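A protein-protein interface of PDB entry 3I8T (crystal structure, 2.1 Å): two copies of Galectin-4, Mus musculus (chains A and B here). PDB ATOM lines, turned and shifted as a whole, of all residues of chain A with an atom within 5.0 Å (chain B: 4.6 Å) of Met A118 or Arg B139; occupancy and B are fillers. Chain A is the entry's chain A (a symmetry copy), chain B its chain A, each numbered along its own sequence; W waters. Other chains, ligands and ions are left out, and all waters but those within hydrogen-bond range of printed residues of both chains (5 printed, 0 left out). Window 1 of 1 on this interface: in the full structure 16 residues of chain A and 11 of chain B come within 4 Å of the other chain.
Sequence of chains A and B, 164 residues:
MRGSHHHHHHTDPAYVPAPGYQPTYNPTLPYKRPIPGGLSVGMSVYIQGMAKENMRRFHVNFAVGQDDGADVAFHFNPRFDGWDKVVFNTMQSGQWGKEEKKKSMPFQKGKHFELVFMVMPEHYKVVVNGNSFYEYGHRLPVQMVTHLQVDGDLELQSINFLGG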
ATOM      1  N   MET A  43      -6.477  10.455  25.761  1.00  0.00           N
ATOM      2  CA  MET A  43      -6.446  11.918  25.684  1.00  0.00           C
ATOM      3  C   MET A  43      -5.390  12.413  24.715  1.00  0.00           C
ATOM      4  O   MET A  43      -4.384  11.718  24.461  1.00  0.00           O
ATOM      5  CB  MET A  43      -6.209  12.530  27.084  1.00  0.00           C
ATOM      6  CG  MET A  43      -7.494  12.510  27.907  1.00  0.00           C
ATOM      7  SD  MET A  43      -7.390  13.323  29.544  1.00  0.00           S
ATOM      8  CE  MET A  43      -6.431  14.789  29.063  1.00  0.00           C
ATOM      9  N   SER A  44      -5.613  13.613  24.184  1.00  0.00           N
ATOM     10  CA  SER A  44      -4.576  14.306  23.440  1.00  0.00           C
ATOM     11  C   SER A  44      -4.456  15.743  23.913  1.00  0.00           C
ATOM     12  O   SER A  44      -5.367  16.274  24.534  1.00  0.00           O
ATOM     13  CB  SER A  44      -4.854  14.272  21.932  1.00  0.00           C
ATOM     14  OG  SER A  44      -6.166  14.709  21.669  1.00  0.00           O
ATOM     15  N   VAL A 116       1.308  18.128  18.791  1.00  0.00           N
ATOM     16  CA  VAL A 116       0.266  17.271  19.315  1.00  0.00           C
ATOM     17  C   VAL A 116       0.859  16.073  20.079  1.00  0.00           C
ATOM     18  O   VAL A 116       1.791  15.423  19.580  1.00  0.00           O
ATOM     19  CB  VAL A 116      -0.671  16.795  18.181  1.00  0.00           C
ATOM     20  CG1 VAL A 116      -1.661  15.770  18.701  1.00  0.00           C
ATOM     21  CG2 VAL A 116      -1.415  17.970  17.542  1.00  0.00           C
ATOM     22  N   PHE A 117       0.328  15.814  21.283  1.00  0.00           N
ATOM     23  CA  PHE A 117       0.672  14.635  22.057  1.00  0.00           C
ATOM     24  C   PHE A 117      -0.552  13.784  22.162  1.00  0.00           C
ATOM     25  O   PHE A 117      -1.593  14.294  22.558  1.00  0.00           O
ATOM     26  CB  PHE A 117       1.082  15.031  23.472  1.00  0.00           C
ATOM     27  CG  PHE A 117       2.269  15.942  23.519  1.00  0.00           C
ATOM     28  CD1 PHE A 117       3.558  15.403  23.507  1.00  0.00           C
ATOM     29  CD2 PHE A 117       2.096  17.357  23.564  1.00  0.00           C
ATOM     30  CE1 PHE A 117       4.704  16.245  23.567  1.00  0.00           C
ATOM     31  CE2 PHE A 117       3.225  18.190  23.626  1.00  0.00           C
ATOM     32  CZ  PHE A 117       4.537  17.618  23.630  1.00  0.00           C
ATOM     33  N   MET A 118      -0.451  12.506  21.806  1.00  0.00           N
ATOM     34  CA  MET A 118      -1.575  11.586  21.935  1.00  0.00           C
ATOM     35  C   MET A 118      -1.196  10.569  23.001  1.00  0.00           C
ATOM     36  O   MET A 118      -0.078  10.068  22.988  1.00  0.00           O
ATOM     37  CB  MET A 118      -1.789  10.849  20.633  1.00  0.00           C
ATOM     38  CG  MET A 118      -2.551  11.677  19.629  1.00  0.00           C
ATOM     39  SD  MET A 118      -2.776  11.000  17.947  1.00  0.00           S
ATOM     40  CE  MET A 118      -1.102  11.182  17.391  1.00  0.00           C
ATOM     41  N   VAL A 119      -2.088  10.297  23.943  1.00  0.00           N
ATOM     42  CA  VAL A 119      -1.705   9.394  25.060  1.00  0.00           C
ATOM     43  C   VAL A 119      -2.240   8.029  24.670  1.00  0.00           C
ATOM     44  O   VAL A 119      -3.453   7.770  24.706  1.00  0.00           O
ATOM     45  CB  VAL A 119      -2.255   9.813  26.468  1.00  0.00           C
ATOM     46  CG1 VAL A 119      -1.667   8.919  27.570  1.00  0.00           C
ATOM     47  CG2 VAL A 119      -1.909  11.330  26.796  1.00  0.00           C
ATOM     48  N   MET A 120      -1.322   7.172  24.252  1.00  0.00           N
ATOM     49  CA  MET A 120      -1.698   5.790  23.966  1.00  0.00           C
ATOM     50  C   MET A 120      -1.373   4.883  25.162  1.00  0.00           C
ATOM     51  O   MET A 120      -0.683   5.293  26.090  1.00  0.00           O
ATOM     52  CB  MET A 120      -1.013   5.360  22.672  1.00  0.00           C
ATOM     53  CG  MET A 120      -1.386   6.393  21.461  1.00  0.00           C
ATOM     54  SD  MET A 120      -0.425   6.084  20.022  1.00  0.00           S
ATOM     55  CE  MET A 120      -1.316   7.173  18.843  1.00  0.00           C
ATOM     56  N   HIS A 123       2.574   4.404  24.969  1.00  0.00           N
ATOM     57  CA  HIS A 123       3.457   5.585  24.820  1.00  0.00           C
ATOM     58  C   HIS A 123       2.698   6.873  24.604  1.00  0.00           C
ATOM     59  O   HIS A 123       1.489   6.863  24.319  1.00  0.00           O
ATOM     60  CB  HIS A 123       4.468   5.339  23.673  1.00  0.00           C
ATOM     61  CG  HIS A 123       3.841   4.791  22.448  1.00  0.00           C
ATOM     62  ND1 HIS A 123       3.909   3.452  22.098  1.00  0.00           N
ATOM     63  CD2 HIS A 123       3.042   5.396  21.528  1.00  0.00           C
ATOM     64  CE1 HIS A 123       3.203   3.264  20.993  1.00  0.00           C
ATOM     65  NE2 HIS A 123       2.680   4.434  20.614  1.00  0.00           N
ATOM     66  N   TYR A 124       3.384   7.998  24.822  1.00  0.00           N
ATOM     67  CA  TYR A 124       2.956   9.268  24.213  1.00  0.00           C
ATOM     68  C   TYR A 124       3.419   9.294  22.775  1.00  0.00           C
ATOM     69  O   TYR A 124       4.600   9.093  22.538  1.00  0.00           O
ATOM     70  CB  TYR A 124       3.654  10.459  24.892  1.00  0.00           C
ATOM     71  CG  TYR A 124       3.354  10.619  26.383  1.00  0.00           C
ATOM     72  CD1 TYR A 124       2.289  11.429  26.827  1.00  0.00           C
ATOM     73  CD2 TYR A 124       4.112   9.970  27.330  1.00  0.00           C
ATOM     74  CE1 TYR A 124       2.054  11.603  28.189  1.00  0.00           C
ATOM     75  CE2 TYR A 124       3.846  10.098  28.668  1.00  0.00           C
ATOM     76  CZ  TYR A 124       2.854  10.954  29.098  1.00  0.00           C
ATOM     77  OH  TYR A 124       2.600  11.060  30.444  1.00  0.00           O
ATOM     78  N   LYS A 125       2.506   9.548  21.818  1.00  0.00           N
ATOM     79  CA  LYS A 125       2.913   9.790  20.436  1.00  0.00           C
ATOM     80  C   LYS A 125       2.993  11.318  20.169  1.00  0.00           C
ATOM     81  O   LYS A 125       2.060  12.060  20.467  1.00  0.00           O
ATOM     82  CB  LYS A 125       2.032   9.004  19.407  1.00  0.00           C
ATOM     83  CG  LYS A 125       2.471   9.234  17.955  1.00  0.00           C
ATOM     84  CD  LYS A 125       1.690   8.425  16.967  1.00  0.00           C
ATOM     85  CE  LYS A 125       2.275   8.561  15.576  1.00  0.00           C
ATOM     86  NZ  LYS A 125       1.427   7.686  14.675  1.00  0.00           N
ATOM     87  N   VAL A 127       3.420  14.398  17.472  1.00  0.00           N
ATOM     88  CA  VAL A 127       3.257  14.740  16.076  1.00  0.00           C
ATOM     89  C   VAL A 127       3.486  16.266  15.951  1.00  0.00           C
ATOM     90  O   VAL A 127       2.883  17.044  16.710  1.00  0.00           O
ATOM     91  CB  VAL A 127       1.833  14.336  15.545  1.00  0.00           C
ATOM     92  CG1 VAL A 127       1.729  14.609  14.041  1.00  0.00           C
ATOM     93  CG2 VAL A 127       1.564  12.815  15.790  1.00  0.00           C
ATOM     94  N   GLY A 130       1.813  18.001  11.836  1.00  0.00           N
ATOM     95  CA  GLY A 130       1.203  16.902  11.075  1.00  0.00           C
ATOM     96  C   GLY A 130       2.116  15.700  10.824  1.00  0.00           C
ATOM     97  O   GLY A 130       1.634  14.653  10.362  1.00  0.00           O
ATOM     98  N   SER A 132       4.395  12.688  12.099  1.00  0.00           N
ATOM     99  CA  SER A 132       4.747  11.863  13.255  1.00  0.00           C
ATOM    100  C   SER A 132       6.230  12.019  13.569  1.00  0.00           C
ATOM    101  O   SER A 132       7.080  12.003  12.664  1.00  0.00           O
ATOM    102  CB  SER A 132       4.408  10.395  13.034  1.00  0.00           C
ATOM    103  OG  SER A 132       3.069  10.305  12.622  1.00  0.00           O
ATOM    104  N   PHE B  88      -2.003   6.893   1.328  1.00  0.00           N
ATOM    105  CA  PHE B  88      -2.589   7.210   2.632  1.00  0.00           C
ATOM    106  C   PHE B  88      -1.980   8.527   3.086  1.00  0.00           C
ATOM    107  O   PHE B  88      -0.753   8.725   2.957  1.00  0.00           O
ATOM    108  CB  PHE B  88      -2.227   6.143   3.692  1.00  0.00           C
ATOM    109  CG  PHE B  88      -2.367   4.713   3.213  1.00  0.00           C
ATOM    110  CD1 PHE B  88      -3.578   4.031   3.360  1.00  0.00           C
ATOM    111  CD2 PHE B  88      -1.291   4.045   2.671  1.00  0.00           C
ATOM    112  CE1 PHE B  88      -3.723   2.679   2.961  1.00  0.00           C
ATOM    113  CE2 PHE B  88      -1.439   2.705   2.230  1.00  0.00           C
ATOM    114  CZ  PHE B  88      -2.688   2.051   2.363  1.00  0.00           C
ATOM    115  N   ASN B  89      -2.807   9.424   3.615  1.00  0.00           N
ATOM    116  CA  ASN B  89      -2.285  10.750   4.033  1.00  0.00           C
ATOM    117  C   ASN B  89      -3.224  11.420   5.043  1.00  0.00           C
ATOM    118  O   ASN B  89      -4.291  10.854   5.377  1.00  0.00           O
ATOM    119  CB  ASN B  89      -1.996  11.681   2.825  1.00  0.00           C
ATOM    120  CG  ASN B  89      -0.796  12.617   3.074  1.00  0.00           C
ATOM    121  OD1 ASN B  89      -0.391  12.831   4.225  1.00  0.00           O
ATOM    122  ND2 ASN B  89      -0.236  13.163   2.008  1.00  0.00           N
ATOM    123  N   THR B  90      -2.790  12.584   5.544  1.00  0.00           N
ATOM    124  CA  THR B  90      -3.515  13.390   6.506  1.00  0.00           C
ATOM    125  C   THR B  90      -3.413  14.806   5.970  1.00  0.00           C
ATOM    126  O   THR B  90      -2.340  15.209   5.512  1.00  0.00           O
ATOM    127  CB  THR B  90      -2.865  13.285   7.937  1.00  0.00           C
ATOM    128  OG1 THR B  90      -3.114  11.973   8.484  1.00  0.00           O
ATOM    129  CG2 THR B  90      -3.429  14.351   8.907  1.00  0.00           C
ATOM    130  N   GLN B  92      -3.747  18.582   7.368  1.00  0.00           N
ATOM    131  CA  GLN B  92      -3.799  19.306   8.636  1.00  0.00           C
ATOM    132  C   GLN B  92      -3.498  20.760   8.367  1.00  0.00           C
ATOM    133  O   GLN B  92      -2.511  21.117   7.664  1.00  0.00           O
ATOM    134  CB  GLN B  92      -2.874  18.688   9.706  1.00  0.00           C
ATOM    135  CG  GLN B  92      -2.690  19.548  10.970  1.00  0.00           C
ATOM    136  CD  GLN B  92      -1.876  18.827  12.040  1.00  0.00           C
ATOM    137  OE1 GLN B  92      -1.875  17.588  12.122  1.00  0.00           O
ATOM    138  NE2 GLN B  92      -1.165  19.591  12.843  1.00  0.00           N
ATOM    139  N   GLY B  97       0.181  15.945   4.385  1.00  0.00           N
ATOM    140  CA  GLY B  97       1.447  15.569   5.010  1.00  0.00           C
ATOM    141  C   GLY B  97       2.253  14.666   4.109  1.00  0.00           C
ATOM    142  O   GLY B  97       2.083  14.687   2.875  1.00  0.00           O
ATOM    143  N   LYS B  98       3.126  13.868   4.725  1.00  0.00           N
ATOM    144  CA  LYS B  98       3.956  12.892   4.005  1.00  0.00           C
ATOM    145  C   LYS B  98       3.121  11.687   3.620  1.00  0.00           C
ATOM    146  O   LYS B  98       2.583  11.018   4.488  1.00  0.00           O
ATOM    147  CB  LYS B  98       5.109  12.409   4.888  1.00  0.00           C
ATOM    148  CG  LYS B  98       6.145  13.473   5.250  1.00  0.00           C
ATOM    149  CD  LYS B  98       6.939  12.973   6.473  1.00  0.00           C
ATOM    150  CE  LYS B  98       8.048  13.926   6.900  1.00  0.00           C
ATOM    151  NZ  LYS B  98       8.521  13.491   8.289  1.00  0.00           N
ATOM    152  N   GLU B 100       2.052   8.072   2.719  1.00  0.00           N
ATOM    153  CA  GLU B 100       2.433   6.689   2.819  1.00  0.00           C
ATOM    154  C   GLU B 100       1.810   6.016   1.611  1.00  0.00           C
ATOM    155  O   GLU B 100       0.810   6.489   1.061  1.00  0.00           O
ATOM    156  CB  GLU B 100       1.936   6.093   4.161  1.00  0.00           C
ATOM    157  CG  GLU B 100       2.776   6.642   5.383  1.00  0.00           C
ATOM    158  CD  GLU B 100       2.156   6.276   6.732  1.00  0.00           C
ATOM    159  OE1 GLU B 100       1.726   5.110   6.907  1.00  0.00           O
ATOM    160  OE2 GLU B 100       2.084   7.150   7.630  1.00  0.00           O
ATOM    161  N   TYR B 136      -2.409   2.380   9.483  1.00  0.00           N
ATOM    162  CA  TYR B 136      -2.011   3.776   9.327  1.00  0.00           C
ATOM    163  C   TYR B 136      -1.967   4.432  10.721  1.00  0.00           C
ATOM    164  O   TYR B 136      -2.990   4.513  11.401  1.00  0.00           O
ATOM    165  CB  TYR B 136      -3.002   4.471   8.425  1.00  0.00           C
ATOM    166  CG  TYR B 136      -2.668   5.937   8.155  1.00  0.00           C
ATOM    167  CD1 TYR B 136      -1.757   6.278   7.133  1.00  0.00           C
ATOM    168  CD2 TYR B 136      -3.282   6.967   8.903  1.00  0.00           C
ATOM    169  CE1 TYR B 136      -1.472   7.626   6.843  1.00  0.00           C
ATOM    170  CE2 TYR B 136      -2.959   8.334   8.654  1.00  0.00           C
ATOM    171  CZ  TYR B 136      -2.086   8.641   7.603  1.00  0.00           C
ATOM    172  OH  TYR B 136      -1.795   9.962   7.288  1.00  0.00           O
ATOM    173  N   GLY B 137      -0.762   4.784  11.178  1.00  0.00           N
ATOM    174  CA  GLY B 137      -0.604   5.388  12.504  1.00  0.00           C
ATOM    175  C   GLY B 137      -1.380   6.692  12.541  1.00  0.00           C
ATOM    176  O   GLY B 137      -1.364   7.492  11.568  1.00  0.00           O
ATOM    177  N   HIS B 138      -1.987   6.961  13.688  1.00  0.00           N
ATOM    178  CA  HIS B 138      -2.747   8.206  13.864  1.00  0.00           C
ATOM    179  C   HIS B 138      -1.818   9.412  13.811  1.00  0.00           C
ATOM    180  O   HIS B 138      -0.776   9.426  14.491  1.00  0.00           O
ATOM    181  CB  HIS B 138      -3.411   8.164  15.230  1.00  0.00           C
ATOM    182  CG  HIS B 138      -4.445   7.097  15.360  1.00  0.00           C
ATOM    183  ND1 HIS B 138      -5.547   7.020  14.536  1.00  0.00           N
ATOM    184  CD2 HIS B 138      -4.573   6.088  16.261  1.00  0.00           C
ATOM    185  CE1 HIS B 138      -6.263   5.960  14.868  1.00  0.00           C
ATOM    186  NE2 HIS B 138      -5.693   5.380  15.912  1.00  0.00           N
ATOM    187  N   ARG B 139      -2.187  10.457  13.061  1.00  0.00           N
ATOM    188  CA  ARG B 139      -1.420  11.704  13.087  1.00  0.00           C
ATOM    189  C   ARG B 139      -2.224  12.824  13.747  1.00  0.00           C
ATOM    190  O   ARG B 139      -1.629  13.707  14.347  1.00  0.00           O
ATOM    191  CB  ARG B 139      -1.035  12.172  11.658  1.00  0.00           C
ATOM    192  CG  ARG B 139      -0.190  11.133  10.882  1.00  0.00           C
ATOM    193  CD  ARG B 139       0.179  11.653   9.566  1.00  0.00           C
ATOM    194  NE  ARG B 139       0.749  10.592   8.724  1.00  0.00           N
ATOM    195  CZ  ARG B 139       1.052  10.759   7.431  1.00  0.00           C
ATOM    196  NH1 ARG B 139       0.844  11.957   6.844  1.00  0.00           N
ATOM    197  NH2 ARG B 139       1.603   9.753   6.732  1.00  0.00           N
ATOM    198  N   LEU B 140      -3.556  12.810  13.594  1.00  0.00           N
ATOM    199  CA  LEU B 140      -4.467  13.736  14.306  1.00  0.00           C
ATOM    200  C   LEU B 140      -5.300  12.887  15.279  1.00  0.00           C
ATOM    201  O   LEU B 140      -5.602  11.760  14.981  1.00  0.00           O
ATOM    202  CB  LEU B 140      -5.439  14.461  13.326  1.00  0.00           C
ATOM    203  CG  LEU B 140      -4.947  15.658  12.535  1.00  0.00           C
ATOM    204  CD1 LEU B 140      -5.969  16.177  11.513  1.00  0.00           C
ATOM    205  CD2 LEU B 140      -4.583  16.789  13.524  1.00  0.00           C
ATOM    206  N   PRO B 141      -5.617  13.410  16.469  1.00  0.00           N
ATOM    207  CA  PRO B 141      -6.408  12.638  17.437  1.00  0.00           C
ATOM    208  C   PRO B 141      -7.757  12.158  16.841  1.00  0.00           C
ATOM    209  O   PRO B 141      -8.459  12.919  16.103  1.00  0.00           O
ATOM    210  CB  PRO B 141      -6.624  13.635  18.591  1.00  0.00           C
ATOM    211  CG  PRO B 141      -5.486  14.654  18.439  1.00  0.00           C
ATOM    212  CD  PRO B 141      -5.219  14.741  16.981  1.00  0.00           C
HETATM  213  O   HOH W   1       0.292  14.651   7.993  1.00  0.00           O
HETATM  214  O   HOH W   2       7.039  11.839   9.882  1.00  0.00           O
HETATM  215  O   HOH W   3       4.041  11.651   9.164  1.00  0.00           O
HETATM  216  O   HOH W   4       3.372  13.819   7.553  1.00  0.00           O
HETATM  217  O   HOH W   5       0.798  18.142  14.571  1.00  0.00           O
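O of His B138 lies within hydrogen-bond range of NZ of Lys A125 (2.8 Å).
N of Val A116 lies within hydrogen-bond range of O of Val A127 (2.8 Å).
OH of Tyr B136 sits close to NE of Arg B139, at 3.0 Å.
OD1 of Asn B89 sits at hydrogen-bond distance from NH1 of Arg B139, at 3.0 Å.
The guanidinium group (NH2) of Arg B139 is in hydrogen-bond range of the backbone carbonyl oxygen (O) of Lys B98, at 2.8 Å.
N of Met A118 is in hydrogen-bond range of O of Lys A125 (2.9 Å).
NH2 of Arg B139 lies within salt-bridge range of OE2 of Glu B100 (2.8 Å).
Pro B141 touches Ser A44 (CB to OG, 3.3 Å).
Val A116 touches Pro B141 (CG1 to CG, 3.99 Å).
CE of Met A118 touches O of His B138, 3.4 Å away.
Arg B139 touches Met A118.
Lys A125 touches Gly B137.
Val A127 touches Arg B139 (CG1 to O, 3.5 Å).
OE1 of Gln B92 touches CA of Gly A130 (3.3 Å).
Arg B139 touches Gly A130 (CD to O, 3.4 Å).
Ser A132 touches Arg B139 (OG to CG, 3.8 Å).
Of the 13 printed residues of chain B, 5 touch a printed residue of chain A.
Of the 13 printed residues of chain A, 7 touch a printed residue of chain B.
Hydrophobic or aromatic side chains of chain A within 4 Å of the printed part of chain B: Val A116, Met A118 and Val A127.
Among the printed residues, 10 pairs touch across the chains.
Among the printed residues, no Asp or Glu carboxylate lies within 4 Å of a Lys or Arg side-chain nitrogen of the other chain.
No position is printed for both chains.
Of the 10 pairs that touch across the chains among the printed residues, none has its exchanged pair printed and touching as well.
Of the printed residues of chain B, Val A116 touches Pro B141 (3.99 Å).
Of the printed residues of chain B, Met A118 touches His B138 and Arg B139.
Of the printed residues of chain B, Lys A125 touches Gly B137 and His B138.
Printed residues of chain B within 4 Å of Ser A132: Arg B139 (3.8 Å).
Of the printed residues of chain A, Gln B92 touches Gly A130 (3.3 Å).
Printed residues of chain A within 4 Å of Gly B137: Lys A125 (3.7 Å).
Printed residues of chain A within 4 Å of Arg B139: Met A118 (3.99 Å), Val A127 (3.5 Å), Gly A130 (3.4 Å) and Ser A132 (3.8 Å).
The nearest printed residue of chain B that does not touch Met A118 is Pro B141 (4.01 Å).
The nearest printed residue of chain A that does not touch Arg B139 is Val A116 (4.8 Å).
Water W1 bridges O of Gly A130 (2.7 Å) and NH1 of Arg B139 (3.0 Å).
Water W2 lies within hydrogen-bond range of the side-chain amino group (NZ) of Lys B98 and the backbone carbonyl oxygen (O) of Ser A132.
Water W4 lies within hydrogen-bond range of N of Lys B98 (2.8 Å), NH1 of Arg B139 (3.2 Å) and O of Gly A130 (3.4 Å).
Water W5 lies within hydrogen-bond range of the backbone NH (N) of Gly A130 (2.9 Å), the side-chain amide nitrogen (NE2) of Gln B92 (3.0 Å) and the backbone carbonyl oxygen (O) of Val A127 (3.2 Å).
Water W3 bridges N of Ser A132 (3.1 Å) and NE of Arg B139 (3.5 Å).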
